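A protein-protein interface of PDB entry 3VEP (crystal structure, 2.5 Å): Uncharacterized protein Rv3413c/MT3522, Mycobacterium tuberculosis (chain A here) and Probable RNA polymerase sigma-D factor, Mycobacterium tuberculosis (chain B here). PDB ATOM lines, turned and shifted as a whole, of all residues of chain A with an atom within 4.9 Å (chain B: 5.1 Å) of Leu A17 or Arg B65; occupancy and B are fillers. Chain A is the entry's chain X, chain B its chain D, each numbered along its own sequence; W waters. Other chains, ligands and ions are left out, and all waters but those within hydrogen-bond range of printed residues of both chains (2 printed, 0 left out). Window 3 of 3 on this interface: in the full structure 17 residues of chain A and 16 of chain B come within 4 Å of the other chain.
Among the printed residues, merely in contact across the chains: Leu A17 with His B69 (3.5 Å), Glu A16 with His B69 (3.6 Å), Asp A21 with Ala B50 (3.6 Å) and Leu A17 with Arg B65 (3.8 Å).
Leu A14 touches none of the printed residues of chain B.
Of the printed residues of chain B, Leu A17 touches Arg B65 (3.8 Å) and His B69 (3.5 Å).
Of the printed residues of chain B, Thr A20 touches His B69 (2.6 Å).
Of the printed residues of chain B, Asp A21 touches Ala B50, Arg B65 and Gln B68.
Val B64 touches none of the printed residues of chain A.
Arg B65 touches just these residues of chain A: Leu A17 and Asp A21.
ND1 of His B69 lies within hydrogen-bond range of OG1 of Thr A20 (2.6 Å).
OD2 of Asp A21 lies within salt-bridge range of NH2 of Arg B65 (3.8 Å).
The side-chain carboxylate (OD1) of Asp A21 is in hydrogen-bond range of the side-chain amide nitrogen (NE2) of Gln B68 (2.8 Å).
Water W2 lies within hydrogen-bond range of O of Arg B65 (2.7 Å), NE2 of Gln B68 (2.8 Å) and O of Leu A17 (2.9 Å).
Water W1 lies within hydrogen-bond range of the backbone NH of Ala B50 (2.9 Å) and the side-chain carboxylate of Asp A21 (2.9 Å).
Of the 10 printed residues of chain B, 4 touch a printed residue of chain A.
Printed residues of chain B that touch a printed residue of chain A: Ala B50, Arg B65, Gln B68 and His B69.
Hydrophobic or aromatic side chains of chain B within 4 Å of the printed part of chain A: Ala B50 and His B69.
Of the 9 printed residues of chain A, 4 touch a printed residue of chain B.
Hydrophobic or aromatic side chains of chain A within 4 Å of the printed part of chain B: Leu A17.
Among the printed residues, 7 pairs touch across the chains.
The backbone carbonyl oxygen (O) of Glu A16 lies within hydrogen-bond range of the side-chain hydroxyl (OG1) of Thr A20 (2.9 Å).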
ATOM      1  N   PRO A  13       0.569 -11.424   7.349  1.00  0.00           N
ATOM      2  CA  PRO A  13       1.262 -11.758   6.101  1.00  0.00           C
ATOM      3  C   PRO A  13       0.498 -11.350   4.851  1.00  0.00           C
ATOM      4  O   PRO A  13       1.116 -11.020   3.845  1.00  0.00           O
ATOM      5  CB  PRO A  13       1.386 -13.283   6.167  1.00  0.00           C
ATOM      6  CG  PRO A  13       0.344 -13.715   7.137  1.00  0.00           C
ATOM      7  CD  PRO A  13       0.257 -12.620   8.143  1.00  0.00           C
ATOM      8  N   LEU A  14      -0.826 -11.379   4.909  1.00  0.00           N
ATOM      9  CA  LEU A  14      -1.641 -11.047   3.749  1.00  0.00           C
ATOM     10  C   LEU A  14      -1.413  -9.622   3.262  1.00  0.00           C
ATOM     11  O   LEU A  14      -1.584  -9.330   2.080  1.00  0.00           O
ATOM     12  CB  LEU A  14      -3.123 -11.283   4.043  1.00  0.00           C
ATOM     13  CG  LEU A  14      -3.718 -12.504   3.343  1.00  0.00           C
ATOM     14  CD1 LEU A  14      -4.460 -12.081   2.094  1.00  0.00           C
ATOM     15  CD2 LEU A  14      -2.616 -13.491   3.000  1.00  0.00           C
ATOM     16  N   ASP A  15      -1.024  -8.735   4.169  1.00  0.00           N
ATOM     17  CA  ASP A  15      -0.764  -7.350   3.800  1.00  0.00           C
ATOM     18  C   ASP A  15       0.585  -7.231   3.100  1.00  0.00           C
ATOM     19  O   ASP A  15       0.834  -6.282   2.362  1.00  0.00           O
ATOM     20  CB  ASP A  15      -0.834  -6.439   5.022  1.00  0.00           C
ATOM     21  CG  ASP A  15      -2.253  -6.202   5.482  1.00  0.00           C
ATOM     22  OD1 ASP A  15      -3.176  -6.682   4.796  1.00  0.00           O
ATOM     23  OD2 ASP A  15      -2.447  -5.542   6.523  1.00  0.00           O
ATOM     24  N   GLU A  16       1.450  -8.207   3.340  1.00  0.00           N
ATOM     25  CA  GLU A  16       2.731  -8.288   2.656  1.00  0.00           C
ATOM     26  C   GLU A  16       2.470  -8.367   1.181  1.00  0.00           C
ATOM     27  O   GLU A  16       3.084  -7.662   0.381  1.00  0.00           O
ATOM     28  CB  GLU A  16       3.401  -9.606   2.984  1.00  0.00           C
ATOM     29  CG  GLU A  16       4.732  -9.492   3.568  1.00  0.00           C
ATOM     30  CD  GLU A  16       4.676  -8.890   4.935  1.00  0.00           C
ATOM     31  OE1 GLU A  16       3.553  -8.557   5.397  1.00  0.00           O
ATOM     32  OE2 GLU A  16       5.766  -8.753   5.535  1.00  0.00           O
ATOM     33  N   LEU A  17       1.586  -9.290   0.821  1.00  0.00           N
ATOM     34  CA  LEU A  17       1.345  -9.581  -0.575  1.00  0.00           C
ATOM     35  C   LEU A  17       0.770  -8.346  -1.245  1.00  0.00           C
ATOM     36  O   LEU A  17       1.272  -7.908  -2.272  1.00  0.00           O
ATOM     37  CB  LEU A  17       0.428 -10.786  -0.714  1.00  0.00           C
ATOM     38  CG  LEU A  17       1.094 -12.185  -0.771  1.00  0.00           C
ATOM     39  CD1 LEU A  17       2.636 -12.252  -0.591  1.00  0.00           C
ATOM     40  CD2 LEU A  17       0.413 -13.227   0.093  1.00  0.00           C
ATOM     41  N   ALA A  18      -0.270  -7.779  -0.640  1.00  0.00           N
ATOM     42  CA  ALA A  18      -0.925  -6.591  -1.177  1.00  0.00           C
ATOM     43  C   ALA A  18       0.096  -5.512  -1.404  1.00  0.00           C
ATOM     44  O   ALA A  18       0.027  -4.784  -2.380  1.00  0.00           O
ATOM     45  CB  ALA A  18      -1.996  -6.081  -0.241  1.00  0.00           C
ATOM     46  N   ARG A  19       1.053  -5.397  -0.497  1.00  0.00           N
ATOM     47  CA  ARG A  19       1.987  -4.290  -0.586  1.00  0.00           C
ATOM     48  C   ARG A  19       3.005  -4.441  -1.721  1.00  0.00           C
ATOM     49  O   ARG A  19       3.360  -3.472  -2.394  1.00  0.00           O
ATOM     50  CB  ARG A  19       2.705  -4.044   0.725  1.00  0.00           C
ATOM     51  CG  ARG A  19       3.998  -3.332   0.459  1.00  0.00           C
ATOM     52  CD  ARG A  19       4.603  -2.663   1.654  1.00  0.00           C
ATOM     53  NE  ARG A  19       3.601  -2.268   2.628  1.00  0.00           N
ATOM     54  CZ  ARG A  19       3.750  -2.461   3.933  1.00  0.00           C
ATOM     55  NH1 ARG A  19       4.852  -3.050   4.387  1.00  0.00           N
ATOM     56  NH2 ARG A  19       2.805  -2.077   4.786  1.00  0.00           N
ATOM     57  N   THR A  20       3.487  -5.658  -1.928  1.00  0.00           N
ATOM     58  CA  THR A  20       4.364  -5.913  -3.060  1.00  0.00           C
ATOM     59  C   THR A  20       3.571  -5.649  -4.369  1.00  0.00           C
ATOM     60  O   THR A  20       4.067  -5.005  -5.310  1.00  0.00           O
ATOM     61  CB  THR A  20       4.959  -7.367  -3.008  1.00  0.00           C
ATOM     62  OG1 THR A  20       5.077  -7.781  -1.654  1.00  0.00           O
ATOM     63  CG2 THR A  20       6.328  -7.414  -3.578  1.00  0.00           C
ATOM     64  N   ASP A  21       2.335  -6.145  -4.419  1.00  0.00           N
ATOM     65  CA  ASP A  21       1.510  -5.986  -5.610  1.00  0.00           C
ATOM     66  C   ASP A  21       1.373  -4.514  -5.944  1.00  0.00           C
ATOM     67  O   ASP A  21       1.513  -4.107  -7.100  1.00  0.00           O
ATOM     68  CB  ASP A  21       0.127  -6.570  -5.378  1.00  0.00           C
ATOM     69  CG  ASP A  21      -0.580  -6.910  -6.653  1.00  0.00           C
ATOM     70  OD1 ASP A  21       0.072  -7.292  -7.641  1.00  0.00           O
ATOM     71  OD2 ASP A  21      -1.812  -6.810  -6.667  1.00  0.00           O
ATOM     72  N   ALA B  50      -1.270  -8.218 -12.004  1.00  0.00           N
ATOM     73  CA  ALA B  50      -1.309  -9.554 -11.418  1.00  0.00           C
ATOM     74  C   ALA B  50      -2.207 -10.561 -12.184  1.00  0.00           C
ATOM     75  O   ALA B  50      -1.737 -11.629 -12.582  1.00  0.00           O
ATOM     76  CB  ALA B  50      -1.707  -9.466  -9.949  1.00  0.00           C
ATOM     77  N   THR B  61      -4.132 -15.964 -10.033  1.00  0.00           N
ATOM     78  CA  THR B  61      -3.719 -14.654  -9.589  1.00  0.00           C
ATOM     79  C   THR B  61      -3.021 -14.729  -8.241  1.00  0.00           C
ATOM     80  O   THR B  61      -2.028 -14.037  -8.013  1.00  0.00           O
ATOM     81  CB  THR B  61      -4.912 -13.708  -9.510  1.00  0.00           C
ATOM     82  OG1 THR B  61      -5.285 -13.316 -10.831  1.00  0.00           O
ATOM     83  CG2 THR B  61      -4.560 -12.472  -8.734  1.00  0.00           C
ATOM     84  N   GLY B  62      -3.531 -15.569  -7.341  1.00  0.00           N
ATOM     85  CA  GLY B  62      -2.912 -15.736  -6.036  1.00  0.00           C
ATOM     86  C   GLY B  62      -1.490 -16.222  -6.175  1.00  0.00           C
ATOM     87  O   GLY B  62      -0.583 -15.737  -5.513  1.00  0.00           O
ATOM     88  N   ALA B  63      -1.295 -17.187  -7.056  1.00  0.00           N
ATOM     89  CA  ALA B  63       0.014 -17.751  -7.298  1.00  0.00           C
ATOM     90  C   ALA B  63       0.990 -16.679  -7.761  1.00  0.00           C
ATOM     91  O   ALA B  63       2.140 -16.635  -7.311  1.00  0.00           O
ATOM     92  CB  ALA B  63      -0.079 -18.867  -8.340  1.00  0.00           C
ATOM     93  N   VAL B  64       0.549 -15.815  -8.675  1.00  0.00           N
ATOM     94  CA  VAL B  64       1.428 -14.753  -9.160  1.00  0.00           C
ATOM     95  C   VAL B  64       1.810 -13.824  -8.018  1.00  0.00           C
ATOM     96  O   VAL B  64       2.975 -13.436  -7.898  1.00  0.00           O
ATOM     97  CB  VAL B  64       0.782 -13.901 -10.302  1.00  0.00           C
ATOM     98  CG1 VAL B  64       1.562 -12.591 -10.526  1.00  0.00           C
ATOM     99  CG2 VAL B  64       0.709 -14.701 -11.556  1.00  0.00           C
ATOM    100  N   ARG B  65       0.823 -13.467  -7.189  1.00  0.00           N
ATOM    101  CA  ARG B  65       1.037 -12.586  -6.049  1.00  0.00           C
ATOM    102  C   ARG B  65       2.056 -13.114  -5.070  1.00  0.00           C
ATOM    103  O   ARG B  65       2.756 -12.337  -4.418  1.00  0.00           O
ATOM    104  CB  ARG B  65      -0.233 -12.431  -5.281  1.00  0.00           C
ATOM    105  CG  ARG B  65      -1.348 -11.791  -6.036  1.00  0.00           C
ATOM    106  CD  ARG B  65      -2.594 -12.044  -5.235  1.00  0.00           C
ATOM    107  NE  ARG B  65      -3.175 -10.818  -4.713  1.00  0.00           N
ATOM    108  CZ  ARG B  65      -3.927 -10.019  -5.452  1.00  0.00           C
ATOM    109  NH1 ARG B  65      -4.127 -10.322  -6.725  1.00  0.00           N
ATOM    110  NH2 ARG B  65      -4.459  -8.919  -4.940  1.00  0.00           N
ATOM    111  N   VAL B  66       2.116 -14.436  -4.946  1.00  0.00           N
ATOM    112  CA  VAL B  66       3.089 -15.049  -4.052  1.00  0.00           C
ATOM    113  C   VAL B  66       4.463 -15.091  -4.706  1.00  0.00           C
ATOM    114  O   VAL B  66       5.459 -14.670  -4.124  1.00  0.00           O
ATOM    115  CB  VAL B  66       2.679 -16.473  -3.618  1.00  0.00           C
ATOM    116  CG1 VAL B  66       3.841 -17.123  -2.920  1.00  0.00           C
ATOM    117  CG2 VAL B  66       1.408 -16.451  -2.725  1.00  0.00           C
ATOM    118  N   ALA B  67       4.499 -15.589  -5.936  1.00  0.00           N
ATOM    119  CA  ALA B  67       5.745 -15.688  -6.681  1.00  0.00           C
ATOM    120  C   ALA B  67       6.441 -14.323  -6.867  1.00  0.00           C
ATOM    121  O   ALA B  67       7.675 -14.221  -6.775  1.00  0.00           O
ATOM    122  CB  ALA B  67       5.488 -16.361  -8.039  1.00  0.00           C
ATOM    123  N   GLN B  68       5.658 -13.279  -7.160  1.00  0.00           N
ATOM    124  CA  GLN B  68       6.245 -11.974  -7.397  1.00  0.00           C
ATOM    125  C   GLN B  68       6.800 -11.421  -6.076  1.00  0.00           C
ATOM    126  O   GLN B  68       7.806 -10.733  -6.081  1.00  0.00           O
ATOM    127  CB  GLN B  68       5.263 -11.015  -8.102  1.00  0.00           C
ATOM    128  CG  GLN B  68       4.359 -10.157  -7.175  1.00  0.00           C
ATOM    129  CD  GLN B  68       3.048  -9.663  -7.850  1.00  0.00           C
ATOM    130  OE1 GLN B  68       2.873  -9.749  -9.080  1.00  0.00           O
ATOM    131  NE2 GLN B  68       2.131  -9.137  -7.030  1.00  0.00           N
ATOM    132  N   HIS B  69       6.140 -11.751  -4.958  1.00  0.00           N
ATOM    133  CA  HIS B  69       6.582 -11.345  -3.640  1.00  0.00           C
ATOM    134  C   HIS B  69       7.879 -12.055  -3.295  1.00  0.00           C
ATOM    135  O   HIS B  69       8.870 -11.429  -2.931  1.00  0.00           O
ATOM    136  CB  HIS B  69       5.536 -11.646  -2.583  1.00  0.00           C
ATOM    137  CG  HIS B  69       5.978 -11.318  -1.203  1.00  0.00           C
ATOM    138  ND1 HIS B  69       6.097 -10.010  -0.746  1.00  0.00           N
ATOM    139  CD2 HIS B  69       6.378 -12.098  -0.164  1.00  0.00           C
ATOM    140  CE1 HIS B  69       6.514 -10.016   0.499  1.00  0.00           C
ATOM    141  NE2 HIS B  69       6.697 -11.278   0.877  1.00  0.00           N
HETATM  142  O   HOH W   1      -1.632  -6.399  -9.824  1.00  0.00           O
HETATM  143  O   HOH W   2       2.487  -9.663  -4.264  1.00  0.00           O
